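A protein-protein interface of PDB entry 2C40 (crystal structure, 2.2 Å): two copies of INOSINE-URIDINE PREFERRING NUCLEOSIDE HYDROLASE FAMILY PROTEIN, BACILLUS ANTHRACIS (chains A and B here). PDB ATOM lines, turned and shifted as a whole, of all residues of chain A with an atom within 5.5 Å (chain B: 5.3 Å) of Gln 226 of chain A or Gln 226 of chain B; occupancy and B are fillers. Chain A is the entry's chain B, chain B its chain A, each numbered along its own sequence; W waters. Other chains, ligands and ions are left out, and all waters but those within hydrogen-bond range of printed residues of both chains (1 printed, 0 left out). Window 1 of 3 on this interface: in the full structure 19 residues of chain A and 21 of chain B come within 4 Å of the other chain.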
ATOM      1  N   LEU A  87      12.557  11.846  18.501  1.00  0.00           N
ATOM      2  CA  LEU A  87      12.162  11.860  19.931  1.00  0.00           C
ATOM      3  C   LEU A  87      11.068  10.815  20.239  1.00  0.00           C
ATOM      4  O   LEU A  87      10.028  10.756  19.536  1.00  0.00           O
ATOM      5  CB  LEU A  87      11.670  13.231  20.428  1.00  0.00           C
ATOM      6  CG  LEU A  87      12.714  14.356  20.419  1.00  0.00           C
ATOM      7  CD1 LEU A  87      12.038  15.683  20.742  1.00  0.00           C
ATOM      8  CD2 LEU A  87      13.917  14.035  21.312  1.00  0.00           C
ATOM      9  N   PRO A  88      11.270  10.020  21.303  1.00  0.00           N
ATOM     10  CA  PRO A  88      10.283   8.995  21.637  1.00  0.00           C
ATOM     11  C   PRO A  88       8.836   9.497  21.660  1.00  0.00           C
ATOM     12  O   PRO A  88       7.959   8.862  21.080  1.00  0.00           O
ATOM     13  CB  PRO A  88      10.722   8.522  23.023  1.00  0.00           C
ATOM     14  CG  PRO A  88      12.202   8.733  23.035  1.00  0.00           C
ATOM     15  CD  PRO A  88      12.400  10.014  22.242  1.00  0.00           C
ATOM     16  N   ILE A  89       8.594  10.642  22.297  1.00  0.00           N
ATOM     17  CA  ILE A  89       7.242  11.259  22.329  1.00  0.00           C
ATOM     18  C   ILE A  89       6.545  11.256  20.959  1.00  0.00           C
ATOM     19  O   ILE A  89       5.310  11.022  20.843  1.00  0.00           O
ATOM     20  CB  ILE A  89       7.334  12.709  22.840  1.00  0.00           C
ATOM     21  CG1 ILE A  89       5.987  13.452  22.790  1.00  0.00           C
ATOM     22  CG2 ILE A  89       8.330  13.520  22.016  1.00  0.00           C
ATOM     23  CD1 ILE A  89       5.168  13.243  24.046  1.00  0.00           C
ATOM     24  N   ILE A 221       5.277  20.519  28.034  1.00  0.00           N
ATOM     25  CA  ILE A 221       6.465  21.194  28.616  1.00  0.00           C
ATOM     26  C   ILE A 221       7.702  20.294  28.504  1.00  0.00           C
ATOM     27  O   ILE A 221       8.811  20.781  28.218  1.00  0.00           O
ATOM     28  CB  ILE A 221       6.271  21.574  30.109  1.00  0.00           C
ATOM     29  CG1 ILE A 221       5.154  22.610  30.296  1.00  0.00           C
ATOM     30  CG2 ILE A 221       7.580  22.101  30.714  1.00  0.00           C
ATOM     31  CD1 ILE A 221       5.563  24.032  29.969  1.00  0.00           C
ATOM     32  N   ASP A 222       7.528  19.002  28.795  1.00  0.00           N
ATOM     33  CA  ASP A 222       8.599  18.012  28.629  1.00  0.00           C
ATOM     34  C   ASP A 222       9.057  17.987  27.172  1.00  0.00           C
ATOM     35  O   ASP A 222      10.246  17.929  26.884  1.00  0.00           O
ATOM     36  CB  ASP A 222       8.110  16.632  29.064  1.00  0.00           C
ATOM     37  CG  ASP A 222       9.200  15.561  29.025  1.00  0.00           C
ATOM     38  OD1 ASP A 222      10.378  15.828  29.370  1.00  0.00           O
ATOM     39  OD2 ASP A 222       8.857  14.430  28.663  1.00  0.00           O
ATOM     40  N   PHE A 223       8.109  18.067  26.254  1.00  0.00           N
ATOM     41  CA  PHE A 223       8.422  18.101  24.822  1.00  0.00           C
ATOM     42  C   PHE A 223       9.205  19.355  24.420  1.00  0.00           C
ATOM     43  O   PHE A 223      10.219  19.257  23.707  1.00  0.00           O
ATOM     44  CB  PHE A 223       7.129  17.984  24.026  1.00  0.00           C
ATOM     45  CG  PHE A 223       7.322  18.095  22.539  1.00  0.00           C
ATOM     46  CD1 PHE A 223       6.784  19.159  21.841  1.00  0.00           C
ATOM     47  CD2 PHE A 223       8.035  17.139  21.850  1.00  0.00           C
ATOM     48  CE1 PHE A 223       6.951  19.291  20.501  1.00  0.00           C
ATOM     49  CE2 PHE A 223       8.206  17.246  20.490  1.00  0.00           C
ATOM     50  CZ  PHE A 223       7.666  18.341  19.810  1.00  0.00           C
ATOM     51  N   LEU A 224       8.737  20.529  24.873  1.00  0.00           N
ATOM     52  CA  LEU A 224       9.489  21.779  24.690  1.00  0.00           C
ATOM     53  C   LEU A 224      10.932  21.653  25.166  1.00  0.00           C
ATOM     54  O   LEU A 224      11.850  22.091  24.493  1.00  0.00           O
ATOM     55  CB  LEU A 224       8.888  22.934  25.479  1.00  0.00           C
ATOM     56  CG  LEU A 224       7.672  23.687  24.990  1.00  0.00           C
ATOM     57  CD1 LEU A 224       7.531  24.930  25.830  1.00  0.00           C
ATOM     58  CD2 LEU A 224       7.811  24.070  23.548  1.00  0.00           C
ATOM     59  N   GLY A 225      11.105  21.134  26.361  1.00  0.00           N
ATOM     60  CA  GLY A 225      12.441  20.940  26.920  1.00  0.00           C
ATOM     61  C   GLY A 225      13.334  19.963  26.153  1.00  0.00           C
ATOM     62  O   GLY A 225      14.527  20.151  26.079  1.00  0.00           O
ATOM     63  N   GLN A 226      12.767  18.899  25.598  1.00  0.00           N
ATOM     64  CA  GLN A 226      13.558  17.985  24.745  1.00  0.00           C
ATOM     65  C   GLN A 226      13.995  18.686  23.478  1.00  0.00           C
ATOM     66  O   GLN A 226      15.148  18.575  23.076  1.00  0.00           O
ATOM     67  CB  GLN A 226      12.770  16.720  24.362  1.00  0.00           C
ATOM     68  CG  GLN A 226      12.590  15.709  25.516  1.00  0.00           C
ATOM     69  CD  GLN A 226      11.461  14.697  25.246  1.00  0.00           C
ATOM     70  OE1 GLN A 226      11.463  13.953  24.239  1.00  0.00           O
ATOM     71  NE2 GLN A 226      10.491  14.662  26.157  1.00  0.00           N
ATOM     72  N   CYS A 227      13.080  19.433  22.860  1.00  0.00           N
ATOM     73  CA  CYS A 227      13.446  20.236  21.696  1.00  0.00           C
ATOM     74  C   CYS A 227      14.652  21.202  21.945  1.00  0.00           C
ATOM     75  O   CYS A 227      15.601  21.248  21.141  1.00  0.00           O
ATOM     76  CB  CYS A 227      12.222  20.980  21.207  1.00  0.00           C
ATOM     77  SG  CYS A 227      11.010  19.838  20.524  1.00  0.00           S
ATOM     78  N   TYR A 228      14.628  21.943  23.055  1.00  0.00           N
ATOM     79  CA  TYR A 228      15.679  22.939  23.300  1.00  0.00           C
ATOM     80  C   TYR A 228      16.948  22.385  23.895  1.00  0.00           C
ATOM     81  O   TYR A 228      17.946  23.089  23.996  1.00  0.00           O
ATOM     82  CB  TYR A 228      15.134  24.103  24.134  1.00  0.00           C
ATOM     83  CG  TYR A 228      14.235  24.932  23.276  1.00  0.00           C
ATOM     84  CD1 TYR A 228      12.871  24.965  23.493  1.00  0.00           C
ATOM     85  CD2 TYR A 228      14.750  25.586  22.165  1.00  0.00           C
ATOM     86  CE1 TYR A 228      12.052  25.701  22.694  1.00  0.00           C
ATOM     87  CE2 TYR A 228      13.957  26.293  21.338  1.00  0.00           C
ATOM     88  CZ  TYR A 228      12.593  26.367  21.605  1.00  0.00           C
ATOM     89  OH  TYR A 228      11.815  27.116  20.773  1.00  0.00           O
ATOM     90  N   ALA A 229      16.927  21.113  24.289  1.00  0.00           N
ATOM     91  CA  ALA A 229      18.165  20.415  24.729  1.00  0.00           C
ATOM     92  C   ALA A 229      19.215  20.281  23.608  1.00  0.00           C
ATOM     93  O   ALA A 229      20.401  20.280  23.836  1.00  0.00           O
ATOM     94  CB  ALA A 229      17.808  19.040  25.285  1.00  0.00           C
ATOM     95  N   ILE A 230      18.703  20.158  22.406  1.00  0.00           N
ATOM     96  CA  ILE A 230      19.426  20.100  21.127  1.00  0.00           C
ATOM     97  C   ILE A 230      20.214  21.403  20.816  1.00  0.00           C
ATOM     98  O   ILE A 230      21.190  21.401  20.102  1.00  0.00           O
ATOM     99  CB  ILE A 230      18.355  19.783  19.976  1.00  0.00           C
ATOM    100  CG1 ILE A 230      17.396  18.642  20.473  1.00  0.00           C
ATOM    101  CG2 ILE A 230      19.024  19.460  18.704  1.00  0.00           C
ATOM    102  CD1 ILE A 230      16.754  17.570  19.501  1.00  0.00           C
ATOM    103  N   LEU B  87      18.769  17.450  29.086  1.00  0.00           N
ATOM    104  CA  LEU B  87      17.481  16.755  29.016  1.00  0.00           C
ATOM    105  C   LEU B  87      16.638  16.937  30.333  1.00  0.00           C
ATOM    106  O   LEU B  87      17.179  16.818  31.453  1.00  0.00           O
ATOM    107  CB  LEU B  87      17.694  15.270  28.697  1.00  0.00           C
ATOM    108  CG  LEU B  87      18.160  14.803  27.316  1.00  0.00           C
ATOM    109  CD1 LEU B  87      18.319  13.319  27.349  1.00  0.00           C
ATOM    110  CD2 LEU B  87      17.222  15.221  26.197  1.00  0.00           C
ATOM    111  N   PRO B  88      15.321  17.231  30.188  1.00  0.00           N
ATOM    112  CA  PRO B  88      14.503  17.559  31.361  1.00  0.00           C
ATOM    113  C   PRO B  88      14.483  16.448  32.425  1.00  0.00           C
ATOM    114  O   PRO B  88      14.582  16.730  33.623  1.00  0.00           O
ATOM    115  CB  PRO B  88      13.129  17.786  30.761  1.00  0.00           C
ATOM    116  CG  PRO B  88      13.416  18.182  29.325  1.00  0.00           C
ATOM    117  CD  PRO B  88      14.520  17.302  28.942  1.00  0.00           C
ATOM    118  N   ILE B  89      14.374  15.202  31.992  1.00  0.00           N
ATOM    119  CA  ILE B  89      14.429  14.075  32.913  1.00  0.00           C
ATOM    120  C   ILE B  89      15.582  14.233  33.929  1.00  0.00           C
ATOM    121  O   ILE B  89      15.421  13.914  35.083  1.00  0.00           O
ATOM    122  CB  ILE B  89      14.458  12.685  32.155  1.00  0.00           C
ATOM    123  CG1 ILE B  89      14.986  11.566  33.019  1.00  0.00           C
ATOM    124  CG2 ILE B  89      15.412  12.665  30.991  1.00  0.00           C
ATOM    125  CD1 ILE B  89      14.094  11.205  34.096  1.00  0.00           C
ATOM    126  N   ILE B 221      13.118   3.706  29.559  1.00  0.00           N
ATOM    127  CA  ILE B 221      13.017   3.481  28.119  1.00  0.00           C
ATOM    128  C   ILE B 221      12.907   4.862  27.399  1.00  0.00           C
ATOM    129  O   ILE B 221      13.621   5.108  26.433  1.00  0.00           O
ATOM    130  CB  ILE B 221      11.807   2.548  27.761  1.00  0.00           C
ATOM    131  CG1 ILE B 221      11.966   1.140  28.350  1.00  0.00           C
ATOM    132  CG2 ILE B 221      11.586   2.452  26.272  1.00  0.00           C
ATOM    133  CD1 ILE B 221      13.071   0.302  27.747  1.00  0.00           C
ATOM    134  N   ASP B 222      12.037   5.743  27.898  1.00  0.00           N
ATOM    135  CA  ASP B 222      11.888   7.103  27.379  1.00  0.00           C
ATOM    136  C   ASP B 222      13.262   7.798  27.445  1.00  0.00           C
ATOM    137  O   ASP B 222      13.694   8.406  26.467  1.00  0.00           O
ATOM    138  CB  ASP B 222      10.850   7.835  28.207  1.00  0.00           C
ATOM    139  CG  ASP B 222      10.492   9.216  27.676  1.00  0.00           C
ATOM    140  OD1 ASP B 222      10.667   9.519  26.462  1.00  0.00           O
ATOM    141  OD2 ASP B 222       9.982  10.000  28.505  1.00  0.00           O
ATOM    142  N   PHE B 223      13.978   7.630  28.558  1.00  0.00           N
ATOM    143  CA  PHE B 223      15.334   8.210  28.686  1.00  0.00           C
ATOM    144  C   PHE B 223      16.333   7.660  27.652  1.00  0.00           C
ATOM    145  O   PHE B 223      17.053   8.447  27.008  1.00  0.00           O
ATOM    146  CB  PHE B 223      15.910   8.003  30.080  1.00  0.00           C
ATOM    147  CG  PHE B 223      17.332   8.531  30.244  1.00  0.00           C
ATOM    148  CD1 PHE B 223      18.403   7.666  30.400  1.00  0.00           C
ATOM    149  CD2 PHE B 223      17.591   9.903  30.246  1.00  0.00           C
ATOM    150  CE1 PHE B 223      19.697   8.142  30.559  1.00  0.00           C
ATOM    151  CE2 PHE B 223      18.900  10.390  30.399  1.00  0.00           C
ATOM    152  CZ  PHE B 223      19.934   9.517  30.553  1.00  0.00           C
ATOM    153  N   LEU B 224      16.371   6.324  27.496  1.00  0.00           N
ATOM    154  CA  LEU B 224      17.155   5.684  26.435  1.00  0.00           C
ATOM    155  C   LEU B 224      16.828   6.259  25.071  1.00  0.00           C
ATOM    156  O   LEU B 224      17.729   6.564  24.314  1.00  0.00           O
ATOM    157  CB  LEU B 224      16.875   4.173  26.334  1.00  0.00           C
ATOM    158  CG  LEU B 224      17.689   3.157  27.063  1.00  0.00           C
ATOM    159  CD1 LEU B 224      16.993   1.766  26.878  1.00  0.00           C
ATOM    160  CD2 LEU B 224      19.148   3.155  26.512  1.00  0.00           C
ATOM    161  N   GLY B 225      15.545   6.349  24.738  1.00  0.00           N
ATOM    162  CA  GLY B 225      15.144   6.942  23.470  1.00  0.00           C
ATOM    163  C   GLY B 225      15.562   8.396  23.238  1.00  0.00           C
ATOM    164  O   GLY B 225      15.934   8.757  22.137  1.00  0.00           O
ATOM    165  N   GLN B 226      15.478   9.234  24.257  1.00  0.00           N
ATOM    166  CA  GLN B 226      15.949  10.627  24.167  1.00  0.00           C
ATOM    167  C   GLN B 226      17.440  10.650  23.878  1.00  0.00           C
ATOM    168  O   GLN B 226      17.896  11.337  22.959  1.00  0.00           O
ATOM    169  CB  GLN B 226      15.634  11.374  25.450  1.00  0.00           C
ATOM    170  CG  GLN B 226      14.135  11.664  25.513  1.00  0.00           C
ATOM    171  CD  GLN B 226      13.686  12.234  26.830  1.00  0.00           C
ATOM    172  OE1 GLN B 226      14.191  13.242  27.272  1.00  0.00           O
ATOM    173  NE2 GLN B 226      12.687  11.613  27.431  1.00  0.00           N
ATOM    174  N   CYS B 227      18.196   9.854  24.626  1.00  0.00           N
ATOM    175  CA  CYS B 227      19.608   9.734  24.382  1.00  0.00           C
ATOM    176  C   CYS B 227      19.921   9.377  22.901  1.00  0.00           C
ATOM    177  O   CYS B 227      20.723  10.056  22.278  1.00  0.00           O
ATOM    178  CB  CYS B 227      20.209   8.757  25.343  1.00  0.00           C
ATOM    179  SG  CYS B 227      20.357   9.476  27.011  1.00  0.00           S
ATOM    180  N   TYR B 228      19.225   8.392  22.318  1.00  0.00           N
ATOM    181  CA  TYR B 228      19.530   7.962  20.947  1.00  0.00           C
ATOM    182  C   TYR B 228      18.963   8.831  19.814  1.00  0.00           C
ATOM    183  O   TYR B 228      19.378   8.693  18.679  1.00  0.00           O
ATOM    184  CB  TYR B 228      19.184   6.480  20.794  1.00  0.00           C
ATOM    185  CG  TYR B 228      20.245   5.637  21.485  1.00  0.00           C
ATOM    186  CD1 TYR B 228      19.941   4.836  22.585  1.00  0.00           C
ATOM    187  CD2 TYR B 228      21.586   5.724  21.071  1.00  0.00           C
ATOM    188  CE1 TYR B 228      20.916   4.104  23.203  1.00  0.00           C
ATOM    189  CE2 TYR B 228      22.553   5.049  21.687  1.00  0.00           C
ATOM    190  CZ  TYR B 228      22.237   4.228  22.775  1.00  0.00           C
ATOM    191  OH  TYR B 228      23.248   3.514  23.378  1.00  0.00           O
ATOM    192  N   ALA B 229      18.062   9.751  20.143  1.00  0.00           N
ATOM    193  CA  ALA B 229      17.535  10.745  19.227  1.00  0.00           C
ATOM    194  C   ALA B 229      18.628  11.698  18.753  1.00  0.00           C
ATOM    195  O   ALA B 229      18.590  12.258  17.663  1.00  0.00           O
ATOM    196  CB  ALA B 229      16.464  11.539  19.951  1.00  0.00           C
ATOM    197  N   ILE B 230      19.558  11.928  19.654  1.00  0.00           N
ATOM    198  CA  ILE B 230      20.785  12.738  19.467  1.00  0.00           C
ATOM    199  C   ILE B 230      21.745  12.154  18.403  1.00  0.00           C
ATOM    200  O   ILE B 230      22.600  12.817  17.861  1.00  0.00           O
ATOM    201  CB  ILE B 230      21.474  12.823  20.884  1.00  0.00           C
ATOM    202  CG1 ILE B 230      20.644  13.791  21.781  1.00  0.00           C
ATOM    203  CG2 ILE B 230      22.914  13.161  20.786  1.00  0.00           C
ATOM    204  CD1 ILE B 230      21.043  13.922  23.330  1.00  0.00           C
HETATM  205  O   HOH W   1      10.358  11.633  24.157  1.00  0.00           O
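CB of Ala 229 of chain B touches CD2 of Leu 87 of chain A, 3.8 Å away.
CB of Pro 88 of chain A touches OD1 of Asp 222 of chain B, at 3.6 Å.
Pro 88 of chain A touches Gly 225 of chain B.
Gln 226 of chain B touches Pro 88 of chain A.
OD1 of Asp 222 of chain A touches CB of Pro 88 of chain B, 3.7 Å away.
CG of Pro 88 of chain B touches C of Gly 225 of chain A, at 3.6 Å.
Gln 226 of chain A touches Pro 88 of chain B.
CG of Gln 226 of chain A touches OE1 of Gln 226 of chain B (3.4 Å).
Ala 229 of chain A touches Leu 87 of chain B.
Printed residues of chain B within 4 Å of Gly 225 of chain A: Pro 88 (3.6 Å).
Tyr 228 of chain A touches none of the printed residues of chain B.
Of the printed residues of chain B, Ala 229 of chain A touches Leu 87 (3.97 Å).
Ile 89 of chain B touches none of the printed residues of chain A.
Gln 226 of chain B touches two residues of chain A.
The nearest residue of chain B that does not touch Gln 226 of chain A is Leu 87 of chain B (4.7 Å).
The nearest residue of chain A that does not touch Gln 226 of chain B is Leu 87 of chain A (4.8 Å).
Hydrophobic or aromatic side chains of chain A within 4 Å of the printed part of chain B: Leu 87, Pro 88 and Ala 229.
Hydrophobic or aromatic side chains of chain B within 4 Å of the printed part of chain A: Leu 87, Pro 88 and Ala 229.
Among the printed residues, 9 pairs touch across the chains.
Among the printed residues, no Asp or Glu carboxylate lies within 4 Å of a Lys or Arg side-chain nitrogen of the other chain.
Pro 88 of chain A touches Asp 222 of chain B, and with the chains exchanged Asp 222 of chain A touches Pro 88 of chain B.
Pro 88 of chain A touches Gly 225 of chain B, and with the chains exchanged Gly 225 of chain A touches Pro 88 of chain B.
Pro 88 of chain A touches Gln 226 of chain B, and with the chains exchanged Gln 226 of chain A touches Pro 88 of chain B.
Gln 226 of chain A touches its own counterpart, Gln 226 of chain B.
Of the 9 pairs that touch across the chains among the printed residues, 9 have their exchanged pair printed and touching as well.
OD1 of Asp 222 of chain B lies within hydrogen-bond range of NE2 of Gln 226 of chain B (3.1 Å).
The side-chain carboxylate (OD2) of Asp 222 of chain A lies within hydrogen-bond range of the side-chain amide nitrogen (NE2) of Gln 226 of chain A (3.0 Å).
Water W1 lies within hydrogen-bond range of the side-chain amide oxygen of Gln 226 of chain A (2.6 Å), the backbone NH of Ile 89 of chain A (2.7 Å) and the side-chain carboxylate of Asp 222 of chain B (3.1 Å).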
